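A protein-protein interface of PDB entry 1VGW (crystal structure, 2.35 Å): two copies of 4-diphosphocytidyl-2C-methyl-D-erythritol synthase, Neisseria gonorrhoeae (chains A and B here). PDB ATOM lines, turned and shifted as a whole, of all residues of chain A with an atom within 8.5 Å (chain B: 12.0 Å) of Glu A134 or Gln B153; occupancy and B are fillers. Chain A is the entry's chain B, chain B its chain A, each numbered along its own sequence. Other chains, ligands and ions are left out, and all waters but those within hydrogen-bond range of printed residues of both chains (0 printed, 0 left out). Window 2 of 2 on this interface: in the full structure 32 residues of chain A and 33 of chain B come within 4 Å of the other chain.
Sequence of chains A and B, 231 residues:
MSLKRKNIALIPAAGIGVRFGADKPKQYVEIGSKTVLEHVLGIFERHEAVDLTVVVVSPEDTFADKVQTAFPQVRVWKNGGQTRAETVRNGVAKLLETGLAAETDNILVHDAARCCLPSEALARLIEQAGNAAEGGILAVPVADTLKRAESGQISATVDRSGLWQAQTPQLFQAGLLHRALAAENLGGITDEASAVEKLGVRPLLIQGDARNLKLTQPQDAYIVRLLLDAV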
ATOM      1  N   ASN A 106      37.058  -5.854  -5.230  1.00  0.00           N
ATOM      2  CA  ASN A 106      35.715  -5.488  -5.628  1.00  0.00           C
ATOM      3  C   ASN A 106      35.617  -4.180  -6.433  1.00  0.00           C
ATOM      4  O   ASN A 106      36.246  -3.159  -6.087  1.00  0.00           O
ATOM      5  CB  ASN A 106      34.851  -5.366  -4.349  1.00  0.00           C
ATOM      6  CG  ASN A 106      34.717  -6.636  -3.576  1.00  0.00           C
ATOM      7  OD1 ASN A 106      34.473  -7.716  -4.123  1.00  0.00           O
ATOM      8  ND2 ASN A 106      34.842  -6.597  -2.236  1.00  0.00           N
ATOM      9  N   GLN A 128      27.661  -6.976   2.891  1.00  0.00           N
ATOM     10  CA  GLN A 128      27.056  -8.223   2.400  1.00  0.00           C
ATOM     11  C   GLN A 128      27.588  -8.727   1.096  1.00  0.00           C
ATOM     12  O   GLN A 128      28.043  -9.884   0.992  1.00  0.00           O
ATOM     13  CB  GLN A 128      25.536  -8.008   2.347  1.00  0.00           C
ATOM     14  CG  GLN A 128      24.996  -7.692   3.744  1.00  0.00           C
ATOM     15  CD  GLN A 128      23.580  -7.192   3.735  1.00  0.00           C
ATOM     16  OE1 GLN A 128      23.126  -6.587   4.712  1.00  0.00           O
ATOM     17  NE2 GLN A 128      22.846  -7.406   2.648  1.00  0.00           N
ATOM     18  N   ALA A 129      27.686  -7.907   0.062  1.00  0.00           N
ATOM     19  CA  ALA A 129      28.194  -8.436  -1.217  1.00  0.00           C
ATOM     20  C   ALA A 129      29.696  -8.373  -1.265  1.00  0.00           C
ATOM     21  O   ALA A 129      30.352  -9.047  -2.076  1.00  0.00           O
ATOM     22  CB  ALA A 129      27.563  -7.652  -2.371  1.00  0.00           C
ATOM     23  N   GLY A 130      30.306  -7.509  -0.452  1.00  0.00           N
ATOM     24  CA  GLY A 130      31.731  -7.337  -0.448  1.00  0.00           C
ATOM     25  C   GLY A 130      32.529  -8.593  -0.069  1.00  0.00           C
ATOM     26  O   GLY A 130      33.705  -8.674  -0.445  1.00  0.00           O
ATOM     27  N   ASN A 131      31.912  -9.531   0.631  1.00  0.00           N
ATOM     28  CA  ASN A 131      32.501 -10.755   1.078  1.00  0.00           C
ATOM     29  C   ASN A 131      31.830 -12.013   0.526  1.00  0.00           C
ATOM     30  O   ASN A 131      31.892 -13.044   1.187  1.00  0.00           O
ATOM     31  CB  ASN A 131      32.490 -10.873   2.627  1.00  0.00           C
ATOM     32  CG  ASN A 131      33.361  -9.816   3.275  1.00  0.00           C
ATOM     33  OD1 ASN A 131      34.584  -9.807   3.107  1.00  0.00           O
ATOM     34  ND2 ASN A 131      32.736  -8.920   4.021  1.00  0.00           N
ATOM     35  N   ALA A 132      31.158 -11.929  -0.598  1.00  0.00           N
ATOM     36  CA  ALA A 132      30.537 -13.088  -1.227  1.00  0.00           C
ATOM     37  C   ALA A 132      31.138 -13.162  -2.632  1.00  0.00           C
ATOM     38  O   ALA A 132      30.967 -12.137  -3.331  1.00  0.00           O
ATOM     39  CB  ALA A 132      29.028 -12.918  -1.330  1.00  0.00           C
ATOM     40  N   ALA A 133      31.652 -14.300  -3.080  1.00  0.00           N
ATOM     41  CA  ALA A 133      32.271 -14.341  -4.402  1.00  0.00           C
ATOM     42  C   ALA A 133      31.327 -13.966  -5.541  1.00  0.00           C
ATOM     43  O   ALA A 133      31.767 -13.559  -6.639  1.00  0.00           O
ATOM     44  CB  ALA A 133      32.936 -15.708  -4.646  1.00  0.00           C
ATOM     45  N   GLU A 134      30.035 -14.224  -5.388  1.00  0.00           N
ATOM     46  CA  GLU A 134      29.048 -13.934  -6.406  1.00  0.00           C
ATOM     47  C   GLU A 134      28.618 -12.460  -6.509  1.00  0.00           C
ATOM     48  O   GLU A 134      27.953 -12.107  -7.481  1.00  0.00           O
ATOM     49  CB  GLU A 134      27.780 -14.802  -6.287  1.00  0.00           C
ATOM     50  CG  GLU A 134      26.945 -14.569  -5.064  1.00  0.00           C
ATOM     51  CD  GLU A 134      27.336 -15.363  -3.836  1.00  0.00           C
ATOM     52  OE1 GLU A 134      28.549 -15.480  -3.527  1.00  0.00           O
ATOM     53  OE2 GLU A 134      26.436 -15.870  -3.109  1.00  0.00           O
ATOM     54  N   GLY A 135      29.087 -11.563  -5.667  1.00  0.00           N
ATOM     55  CA  GLY A 135      28.746 -10.154  -5.794  1.00  0.00           C
ATOM     56  C   GLY A 135      27.280  -9.919  -5.436  1.00  0.00           C
ATOM     57  O   GLY A 135      26.606 -10.854  -4.984  1.00  0.00           O
ATOM     58  N   GLY A 136      26.788  -8.732  -5.766  1.00  0.00           N
ATOM     59  CA  GLY A 136      25.415  -8.392  -5.347  1.00  0.00           C
ATOM     60  C   GLY A 136      25.115  -6.934  -5.715  1.00  0.00           C
ATOM     61  O   GLY A 136      25.970  -6.241  -6.235  1.00  0.00           O
ATOM     62  N   ILE A 137      23.813  -6.537  -5.631  1.00  0.00           N
ATOM     63  CA  ILE A 137      23.450  -5.198  -6.036  1.00  0.00           C
ATOM     64  C   ILE A 137      22.449  -4.597  -5.070  1.00  0.00           C
ATOM     65  O   ILE A 137      21.781  -5.295  -4.327  1.00  0.00           O
ATOM     66  CB  ILE A 137      22.786  -5.151  -7.434  1.00  0.00           C
ATOM     67  CG1 ILE A 137      21.382  -5.784  -7.371  1.00  0.00           C
ATOM     68  CG2 ILE A 137      23.622  -5.817  -8.517  1.00  0.00           C
ATOM     69  CD1 ILE A 137      20.659  -5.796  -8.712  1.00  0.00           C
ATOM     70  N   GLY A 162       7.706 -11.672  -5.642  1.00  0.00           N
ATOM     71  CA  GLY A 162       9.130 -11.850  -5.674  1.00  0.00           C
ATOM     72  C   GLY A 162       9.899 -10.960  -6.621  1.00  0.00           C
ATOM     73  O   GLY A 162      11.114 -11.246  -6.793  1.00  0.00           O
ATOM     74  N   TRP A 164      11.845  -7.363  -7.964  1.00  0.00           N
ATOM     75  CA  TRP A 164      12.640  -6.266  -7.463  1.00  0.00           C
ATOM     76  C   TRP A 164      13.108  -5.293  -8.549  1.00  0.00           C
ATOM     77  O   TRP A 164      13.434  -5.678  -9.673  1.00  0.00           O
ATOM     78  CB  TRP A 164      13.955  -6.821  -6.787  1.00  0.00           C
ATOM     79  CG  TRP A 164      13.693  -7.646  -5.577  1.00  0.00           C
ATOM     80  CD1 TRP A 164      13.099  -8.888  -5.545  1.00  0.00           C
ATOM     81  CD2 TRP A 164      14.012  -7.359  -4.208  1.00  0.00           C
ATOM     82  NE1 TRP A 164      12.924  -9.306  -4.267  1.00  0.00           N
ATOM     83  CE2 TRP A 164      13.498  -8.409  -3.419  1.00  0.00           C
ATOM     84  CE3 TRP A 164      14.610  -6.286  -3.567  1.00  0.00           C
ATOM     85  CZ2 TRP A 164      13.588  -8.435  -2.031  1.00  0.00           C
ATOM     86  CZ3 TRP A 164      14.729  -6.310  -2.180  1.00  0.00           C
ATOM     87  CH2 TRP A 164      14.226  -7.383  -1.424  1.00  0.00           C
ATOM     88  N   LEU A 171      28.122  -4.406  -7.278  1.00  0.00           N
ATOM     89  CA  LEU A 171      29.468  -4.810  -6.829  1.00  0.00           C
ATOM     90  C   LEU A 171      29.924  -6.181  -7.236  1.00  0.00           C
ATOM     91  O   LEU A 171      29.352  -7.185  -6.759  1.00  0.00           O
ATOM     92  CB  LEU A 171      29.491  -4.603  -5.326  1.00  0.00           C
ATOM     93  CG  LEU A 171      30.237  -5.335  -4.282  1.00  0.00           C
ATOM     94  CD1 LEU A 171      31.286  -6.348  -4.699  1.00  0.00           C
ATOM     95  CD2 LEU A 171      30.786  -4.404  -3.218  1.00  0.00           C
ATOM     96  N   PHE A 172      30.974  -6.280  -8.058  1.00  0.00           N
ATOM     97  CA  PHE A 172      31.568  -7.526  -8.477  1.00  0.00           C
ATOM     98  C   PHE A 172      33.106  -7.534  -8.439  1.00  0.00           C
ATOM     99  O   PHE A 172      33.761  -6.483  -8.547  1.00  0.00           O
ATOM    100  CB  PHE A 172      31.110  -7.887  -9.926  1.00  0.00           C
ATOM    101  CG  PHE A 172      29.614  -8.054  -9.996  1.00  0.00           C
ATOM    102  CD1 PHE A 172      28.841  -7.053 -10.612  1.00  0.00           C
ATOM    103  CD2 PHE A 172      28.960  -9.094  -9.360  1.00  0.00           C
ATOM    104  CE1 PHE A 172      27.458  -7.179 -10.583  1.00  0.00           C
ATOM    105  CE2 PHE A 172      27.593  -9.239  -9.361  1.00  0.00           C
ATOM    106  CZ  PHE A 172      26.828  -8.225  -9.994  1.00  0.00           C
ATOM    107  N   GLN A 173      33.686  -8.721  -8.289  1.00  0.00           N
ATOM    108  CA  GLN A 173      35.131  -8.936  -8.333  1.00  0.00           C
ATOM    109  C   GLN A 173      35.622  -8.462  -9.713  1.00  0.00           C
ATOM    110  O   GLN A 173      34.959  -8.797 -10.711  1.00  0.00           O
ATOM    111  CB  GLN A 173      35.466 -10.459  -8.233  1.00  0.00           C
ATOM    112  CG  GLN A 173      35.333 -11.042  -6.830  1.00  0.00           C
ATOM    113  CD  GLN A 173      35.676 -12.537  -6.847  1.00  0.00           C
ATOM    114  OE1 GLN A 173      36.859 -12.904  -6.946  1.00  0.00           O
ATOM    115  NE2 GLN A 173      34.633 -13.364  -6.880  1.00  0.00           N
ATOM    116  N   LEU A 176      35.911 -11.485 -12.290  1.00  0.00           N
ATOM    117  CA  LEU A 176      34.584 -11.963 -12.688  1.00  0.00           C
ATOM    118  C   LEU A 176      33.846 -10.964 -13.594  1.00  0.00           C
ATOM    119  O   LEU A 176      33.218 -11.330 -14.606  1.00  0.00           O
ATOM    120  CB  LEU A 176      33.744 -12.183 -11.407  1.00  0.00           C
ATOM    121  CG  LEU A 176      32.299 -12.582 -11.613  1.00  0.00           C
ATOM    122  CD1 LEU A 176      32.167 -13.902 -12.369  1.00  0.00           C
ATOM    123  CD2 LEU A 176      31.572 -12.680 -10.262  1.00  0.00           C
ATOM    124  N   ALA A 193      24.815  -6.947 -13.405  1.00  0.00           N
ATOM    125  CA  ALA A 193      24.317  -8.189 -12.880  1.00  0.00           C
ATOM    126  C   ALA A 193      23.871  -9.142 -13.969  1.00  0.00           C
ATOM    127  O   ALA A 193      24.216 -10.326 -13.970  1.00  0.00           O
ATOM    128  CB  ALA A 193      23.218  -7.977 -11.855  1.00  0.00           C
ATOM    129  N   VAL A 196      26.695 -10.940 -15.384  1.00  0.00           N
ATOM    130  CA  VAL A 196      27.237 -11.922 -14.442  1.00  0.00           C
ATOM    131  C   VAL A 196      26.343 -13.159 -14.427  1.00  0.00           C
ATOM    132  O   VAL A 196      26.863 -14.269 -14.527  1.00  0.00           O
ATOM    133  CB  VAL A 196      27.505 -11.329 -13.063  1.00  0.00           C
ATOM    134  CG1 VAL A 196      27.749 -12.397 -11.998  1.00  0.00           C
ATOM    135  CG2 VAL A 196      28.796 -10.463 -13.109  1.00  0.00           C
ATOM    136  N   GLU A 197      25.021 -13.022 -14.384  1.00  0.00           N
ATOM    137  CA  GLU A 197      24.057 -14.128 -14.380  1.00  0.00           C
ATOM    138  C   GLU A 197      24.190 -15.090 -15.568  1.00  0.00           C
ATOM    139  O   GLU A 197      23.918 -16.285 -15.463  1.00  0.00           O
ATOM    140  CB  GLU A 197      22.622 -13.608 -14.378  1.00  0.00           C
ATOM    141  CG  GLU A 197      22.155 -12.744 -13.235  1.00  0.00           C
ATOM    142  CD  GLU A 197      21.058 -11.755 -13.658  1.00  0.00           C
ATOM    143  OE1 GLU A 197      20.205 -12.088 -14.533  1.00  0.00           O
ATOM    144  OE2 GLU A 197      21.020 -10.618 -13.156  1.00  0.00           O
ATOM    145  N   GLY A 200      26.249 -18.206 -15.127  1.00  0.00           N
ATOM    146  CA  GLY A 200      25.728 -19.204 -14.202  1.00  0.00           C
ATOM    147  C   GLY A 200      25.929 -18.764 -12.762  1.00  0.00           C
ATOM    148  O   GLY A 200      25.732 -19.544 -11.838  1.00  0.00           O
ATOM    149  N   VAL A 201      26.280 -17.486 -12.529  1.00  0.00           N
ATOM    150  CA  VAL A 201      26.484 -17.009 -11.153  1.00  0.00           C
ATOM    151  C   VAL A 201      25.245 -16.196 -10.739  1.00  0.00           C
ATOM    152  O   VAL A 201      24.880 -15.320 -11.543  1.00  0.00           O
ATOM    153  CB  VAL A 201      27.689 -16.039 -11.123  1.00  0.00           C
ATOM    154  CG1 VAL A 201      27.857 -15.440  -9.734  1.00  0.00           C
ATOM    155  CG2 VAL A 201      28.962 -16.622 -11.665  1.00  0.00           C
ATOM    156  N   ARG A 202      24.734 -16.297  -9.560  1.00  0.00           N
ATOM    157  CA  ARG A 202      23.588 -15.600  -9.034  1.00  0.00           C
ATOM    158  C   ARG A 202      23.951 -14.558  -7.985  1.00  0.00           C
ATOM    159  O   ARG A 202      24.106 -14.913  -6.791  1.00  0.00           O
ATOM    160  CB  ARG A 202      22.674 -16.630  -8.356  1.00  0.00           C
ATOM    161  CG  ARG A 202      22.064 -17.675  -9.329  1.00  0.00           C
ATOM    162  CD  ARG A 202      21.031 -18.451  -8.481  1.00  0.00           C
ATOM    163  NE  ARG A 202      19.979 -19.033  -9.265  1.00  0.00           N
ATOM    164  CZ  ARG A 202      18.869 -19.543  -8.703  1.00  0.00           C
ATOM    165  NH1 ARG A 202      18.694 -19.497  -7.401  1.00  0.00           N
ATOM    166  NH2 ARG A 202      17.991 -20.116  -9.499  1.00  0.00           N
ATOM    167  N   PRO A 203      23.937 -13.268  -8.318  1.00  0.00           N
ATOM    168  CA  PRO A 203      24.343 -12.231  -7.349  1.00  0.00           C
ATOM    169  C   PRO A 203      23.343 -12.044  -6.241  1.00  0.00           C
ATOM    170  O   PRO A 203      22.157 -12.364  -6.419  1.00  0.00           O
ATOM    171  CB  PRO A 203      24.531 -10.985  -8.185  1.00  0.00           C
ATOM    172  CG  PRO A 203      24.727 -11.477  -9.571  1.00  0.00           C
ATOM    173  CD  PRO A 203      23.811 -12.697  -9.675  1.00  0.00           C
ATOM    174  N   LEU A 204      23.788 -11.601  -5.060  1.00  0.00           N
ATOM    175  CA  LEU A 204      22.835 -11.359  -3.966  1.00  0.00           C
ATOM    176  C   LEU A 204      21.997 -10.107  -4.266  1.00  0.00           C
ATOM    177  O   LEU A 204      22.430  -9.221  -5.019  1.00  0.00           O
ATOM    178  CB  LEU A 204      23.549 -11.145  -2.620  1.00  0.00           C
ATOM    179  CG  LEU A 204      24.568 -12.127  -2.112  1.00  0.00           C
ATOM    180  CD1 LEU A 204      25.308 -11.590  -0.884  1.00  0.00           C
ATOM    181  CD2 LEU A 204      23.917 -13.446  -1.699  1.00  0.00           C
ATOM    182  N   LEU A 205      20.830  -9.995  -3.646  1.00  0.00           N
ATOM    183  CA  LEU A 205      20.006  -8.792  -3.723  1.00  0.00           C
ATOM    184  C   LEU A 205      20.056  -8.138  -2.313  1.00  0.00           C
ATOM    185  O   LEU A 205      19.604  -8.767  -1.350  1.00  0.00           O
ATOM    186  CB  LEU A 205      18.542  -9.032  -4.075  1.00  0.00           C
ATOM    187  CG  LEU A 205      18.214  -9.341  -5.527  1.00  0.00           C
ATOM    188  CD1 LEU A 205      16.923 -10.138  -5.636  1.00  0.00           C
ATOM    189  CD2 LEU A 205      18.148  -8.098  -6.405  1.00  0.00           C
ATOM    190  N   ILE A 206      20.605  -6.935  -2.246  1.00  0.00           N
ATOM    191  CA  ILE A 206      20.708  -6.175  -0.984  1.00  0.00           C
ATOM    192  C   ILE A 206      19.773  -4.951  -1.042  1.00  0.00           C
ATOM    193  O   ILE A 206      19.586  -4.265  -2.061  1.00  0.00           O
ATOM    194  CB  ILE A 206      22.153  -5.759  -0.766  1.00  0.00           C
ATOM    195  CG1 ILE A 206      23.014  -7.035  -0.448  1.00  0.00           C
ATOM    196  CG2 ILE A 206      22.384  -4.730   0.298  1.00  0.00           C
ATOM    197  CD1 ILE A 206      23.992  -7.254  -1.602  1.00  0.00           C
ATOM    198  N   LEU B 146      14.435  -5.184 -14.041  1.00  0.00           N
ATOM    199  CA  LEU B 146      13.748  -5.964 -13.035  1.00  0.00           C
ATOM    200  C   LEU B 146      14.410  -7.335 -12.845  1.00  0.00           C
ATOM    201  O   LEU B 146      14.826  -7.977 -13.817  1.00  0.00           O
ATOM    202  CB  LEU B 146      12.295  -6.208 -13.472  1.00  0.00           C
ATOM    203  CG  LEU B 146      11.331  -5.052 -13.558  1.00  0.00           C
ATOM    204  CD1 LEU B 146      10.026  -5.546 -14.241  1.00  0.00           C
ATOM    205  CD2 LEU B 146      10.992  -4.533 -12.157  1.00  0.00           C
ATOM    206  N   LYS B 147      14.364  -7.872 -11.631  1.00  0.00           N
ATOM    207  CA  LYS B 147      14.955  -9.150 -11.317  1.00  0.00           C
ATOM    208  C   LYS B 147      13.965  -9.985 -10.474  1.00  0.00           C
ATOM    209  O   LYS B 147      13.232  -9.422  -9.676  1.00  0.00           O
ATOM    210  CB  LYS B 147      16.224  -9.004 -10.470  1.00  0.00           C
ATOM    211  CG  LYS B 147      17.341  -8.094 -10.869  1.00  0.00           C
ATOM    212  CD  LYS B 147      17.922  -8.433 -12.263  1.00  0.00           C
ATOM    213  CE  LYS B 147      19.217  -7.707 -12.470  1.00  0.00           C
ATOM    214  NZ  LYS B 147      19.887  -7.835 -13.762  1.00  0.00           N
ATOM    215  N   ARG B 148      14.033 -11.307 -10.615  1.00  0.00           N
ATOM    216  CA  ARG B 148      13.222 -12.187  -9.760  1.00  0.00           C
ATOM    217  C   ARG B 148      14.133 -12.765  -8.676  1.00  0.00           C
ATOM    218  O   ARG B 148      15.225 -13.236  -8.985  1.00  0.00           O
ATOM    219  CB  ARG B 148      12.628 -13.310 -10.635  1.00  0.00           C
ATOM    220  CG  ARG B 148      11.709 -14.280  -9.919  1.00  0.00           C
ATOM    221  CD  ARG B 148      11.000 -15.228 -10.934  1.00  0.00           C
ATOM    222  NE  ARG B 148       9.818 -14.462 -11.487  1.00  0.00           N
ATOM    223  CZ  ARG B 148       9.717 -14.335 -12.808  1.00  0.00           C
ATOM    224  NH1 ARG B 148       8.693 -13.651 -13.341  1.00  0.00           N
ATOM    225  NH2 ARG B 148      10.639 -14.936 -13.582  1.00  0.00           N
ATOM    226  N   ALA B 149      13.749 -12.776  -7.433  1.00  0.00           N
ATOM    227  CA  ALA B 149      14.503 -13.258  -6.315  1.00  0.00           C
ATOM    228  C   ALA B 149      14.054 -14.659  -5.879  1.00  0.00           C
ATOM    229  O   ALA B 149      12.872 -14.948  -5.969  1.00  0.00           O
ATOM    230  CB  ALA B 149      14.267 -12.357  -5.088  1.00  0.00           C
ATOM    231  N   GLU B 150      15.028 -15.429  -5.364  1.00  0.00           N
ATOM    232  CA  GLU B 150      14.667 -16.763  -4.867  1.00  0.00           C
ATOM    233  C   GLU B 150      14.813 -16.765  -3.363  1.00  0.00           C
ATOM    234  O   GLU B 150      13.771 -16.793  -2.661  1.00  0.00           O
ATOM    235  CB  GLU B 150      15.351 -17.890  -5.582  1.00  0.00           C
ATOM    236  CG  GLU B 150      14.360 -19.021  -5.924  1.00  0.00           C
ATOM    237  CD  GLU B 150      14.860 -19.959  -6.991  1.00  0.00           C
ATOM    238  OE1 GLU B 150      15.620 -20.895  -6.636  1.00  0.00           O
ATOM    239  OE2 GLU B 150      14.482 -19.789  -8.173  1.00  0.00           O
ATOM    240  N   SER B 151      16.017 -16.629  -2.823  1.00  0.00           N
ATOM    241  CA  SER B 151      16.074 -16.518  -1.335  1.00  0.00           C
ATOM    242  C   SER B 151      17.143 -15.481  -0.989  1.00  0.00           C
ATOM    243  O   SER B 151      18.062 -15.746  -0.202  1.00  0.00           O
ATOM    244  CB  SER B 151      16.383 -17.829  -0.656  1.00  0.00           C
ATOM    245  OG  SER B 151      15.574 -18.899  -1.037  1.00  0.00           O
ATOM    246  N   GLY B 152      17.091 -14.349  -1.668  1.00  0.00           N
ATOM    247  CA  GLY B 152      18.063 -13.269  -1.468  1.00  0.00           C
ATOM    248  C   GLY B 152      18.980 -13.242  -2.704  1.00  0.00           C
ATOM    249  O   GLY B 152      19.854 -12.385  -2.821  1.00  0.00           O
ATOM    250  N   GLN B 153      18.737 -14.196  -3.605  1.00  0.00           N
ATOM    251  CA  GLN B 153      19.587 -14.214  -4.804  1.00  0.00           C
ATOM    252  C   GLN B 153      18.722 -13.958  -6.040  1.00  0.00           C
ATOM    253  O   GLN B 153      17.536 -14.270  -5.968  1.00  0.00           O
ATOM    254  CB  GLN B 153      20.299 -15.561  -4.952  1.00  0.00           C
ATOM    255  CG  GLN B 153      21.320 -15.854  -3.869  1.00  0.00           C
ATOM    256  CD  GLN B 153      22.344 -16.911  -4.290  1.00  0.00           C
ATOM    257  OE1 GLN B 153      21.967 -18.008  -4.713  1.00  0.00           O
ATOM    258  NE2 GLN B 153      23.618 -16.517  -4.220  1.00  0.00           N
ATOM    259  N   ILE B 154      19.339 -13.598  -7.140  1.00  0.00           N
ATOM    260  CA  ILE B 154      18.658 -13.372  -8.400  1.00  0.00           C
ATOM    261  C   ILE B 154      18.598 -14.690  -9.202  1.00  0.00           C
ATOM    262  O   ILE B 154      19.643 -15.247  -9.612  1.00  0.00           O
ATOM    263  CB  ILE B 154      19.411 -12.310  -9.219  1.00  0.00           C
ATOM    264  CG1 ILE B 154      19.512 -10.977  -8.505  1.00  0.00           C
ATOM    265  CG2 ILE B 154      18.911 -12.197 -10.637  1.00  0.00           C
ATOM    266  CD1 ILE B 154      20.362  -9.944  -9.297  1.00  0.00           C
ATOM    267  N   SER B 155      17.387 -15.129  -9.514  1.00  0.00           N
ATOM    268  CA  SER B 155      17.101 -16.297 -10.329  1.00  0.00           C
ATOM    269  C   SER B 155      16.823 -15.922 -11.781  1.00  0.00           C
ATOM    270  O   SER B 155      16.771 -16.772 -12.670  1.00  0.00           O
ATOM    271  CB  SER B 155      15.889 -17.068  -9.819  1.00  0.00           C
ATOM    272  OG  SER B 155      14.789 -16.172  -9.596  1.00  0.00           O
ATOM    273  N   ALA B 156      16.584 -14.628 -12.040  1.00  0.00           N
ATOM    274  CA  ALA B 156      16.380 -14.198 -13.421  1.00  0.00           C
ATOM    275  C   ALA B 156      16.179 -12.684 -13.554  1.00  0.00           C
ATOM    276  O   ALA B 156      15.723 -12.078 -12.590  1.00  0.00           O
ATOM    277  CB  ALA B 156      15.070 -14.867 -13.940  1.00  0.00           C
ATOM    278  N   THR B 157      16.519 -12.183 -14.737  1.00  0.00           N
ATOM    279  CA  THR B 157      16.225 -10.789 -15.103  1.00  0.00           C
ATOM    280  C   THR B 157      14.938 -10.760 -15.951  1.00  0.00           C
ATOM    281  O   THR B 157      14.821 -11.536 -16.916  1.00  0.00           O
ATOM    282  CB  THR B 157      17.383 -10.164 -15.879  1.00  0.00           C
ATOM    283  OG1 THR B 157      18.390  -9.713 -14.931  1.00  0.00           O
ATOM    284  CG2 THR B 157      16.937  -8.964 -16.696  1.00  0.00           C
ATOM    285  N   VAL B 158      13.887 -10.039 -15.525  1.00  0.00           N
ATOM    286  CA  VAL B 158      12.646 -10.067 -16.353  1.00  0.00           C
ATOM    287  C   VAL B 158      12.536  -8.830 -17.217  1.00  0.00           C
ATOM    288  O   VAL B 158      12.848  -7.714 -16.782  1.00  0.00           O
ATOM    289  CB  VAL B 158      11.401 -10.470 -15.627  1.00  0.00           C
ATOM    290  CG1 VAL B 158      11.698 -11.101 -14.250  1.00  0.00           C
ATOM    291  CG2 VAL B 158      10.324  -9.422 -15.531  1.00  0.00           C
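The backbone carbonyl oxygen (O) of Lys B147 sits at hydrogen-bond distance from the backbone NH (N) of Trp A164.
The side-chain carboxylate (OE2) of Glu A197 lies within salt-bridge range of the side-chain amino group (NZ) of Lys B147 (3.1 Å).
N of Ala B149 sits at hydrogen-bond distance from O of Gly A162.
The side-chain carboxylate of Glu B150 lies within salt-bridge range of the guanidinium group of Arg A202, at 3.5 Å.
O of Gly B152 lies within hydrogen-bond range of N of Leu A205.
NE2 of Gln B153 lies within hydrogen-bond range of OE2 of Glu A134.
The backbone carbonyl oxygen of Arg A202 lies within hydrogen-bond range of the side-chain amide nitrogen of Gln B153 (3.1 Å).
The backbone NH (N) of Ile B154 is in hydrogen-bond range of the backbone carbonyl oxygen (O) of Pro A203, 3.2 Å away.
OE1 of Glu A197 is in hydrogen-bond range of OG1 of Thr B157 (3.0 Å).
The backbone carbonyl oxygen of Leu B146 lies within hydrogen-bond range of the backbone NH of Val B158.
The side-chain hydroxyl (OG1) of Thr B157 is in hydrogen-bond range of the side-chain amino group (NZ) of Lys B147, at 2.7 Å.
O of Arg B148 sits at hydrogen-bond distance from N of Ser B155, 2.9 Å away.
The backbone NH (N) of Arg B148 lies within hydrogen-bond range of the backbone carbonyl oxygen (O) of Ala B156 (2.7 Å).
The backbone NH (N) of Leu A204 lies within hydrogen-bond range of the backbone carbonyl oxygen (O) of Gly A135, 2.9 Å away.
The backbone NH (N) of Ile A137 sits at hydrogen-bond distance from the backbone carbonyl oxygen (O) of Leu A204 (3.1 Å).
Among the printed residues, merely in contact across the chains: Gly A162 with Arg B148 (3.8 Å), Trp A164 with Leu B146 (3.4 Å), Trp A164 with Ala B149 (3.4 Å), Ala A193 with Lys B147 (3.8 Å), Glu A197 with Ile B154 (3.6 Å), Arg A202 with Ile B154 (3.4 Å), Arg A202 with Ser B155 (3.7 Å), Pro A203 with Gln B153 (3.6 Å), Leu A204 with Gly B152 (3.4 Å), Leu A204 with Gln B153 (3.98 Å), Leu A205 with Ala B149 (3.5 Å) and Leu A205 with Ile B154 (3.6 Å).
Ala A132 touches none of the printed residues of chain B.
Glu A134 touches just one residue of chain B: Gln B153.
No residue of chain B comes within 4 Å of Gly A135.
Of the printed residues of chain B, Trp A164 touches Leu B146, Lys B147 and Ala B149.
Leu A171 touches none of the printed residues of chain B.
Gln A173 touches none of the printed residues of chain B.
Pro A203 touches two residues of chain B.
Of the printed residues of chain B, Leu A205 touches Ala B149 (3.5 Å), Gly B152 (2.7 Å) and Ile B154 (3.6 Å).
Printed residues of chain A within 4 Å of Ala B149: Gly A162 (3.1 Å), Trp A164 (3.4 Å) and Leu A205 (3.5 Å).
Gly B152 touches just these residues of chain A: Leu A204 and Leu A205.
Printed residues of chain A within 4 Å of Gln B153: Glu A134 (3.1 Å), Arg A202 (3.1 Å), Pro A203 (3.6 Å) and Leu A204 (3.98 Å).
Of the printed residues of chain A, Ile B154 touches Glu A197 (3.6 Å), Arg A202 (3.4 Å), Pro A203 (3.2 Å) and Leu A205 (3.6 Å).
Hydrophobic or aromatic side chains of chain B that line the printed part of chain A: Leu B146, Ala B149 and Ile B154.
Of the 27 printed residues of chain A, 9 touch a printed residue of chain B.
Hydrophobic or aromatic side chains of chain A that line the printed part of chain B: Trp A164, Ala A193, Leu A204 and Leu A205.
Among the printed residues, 21 pairs touch across the chains.
No position is printed for both chains.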
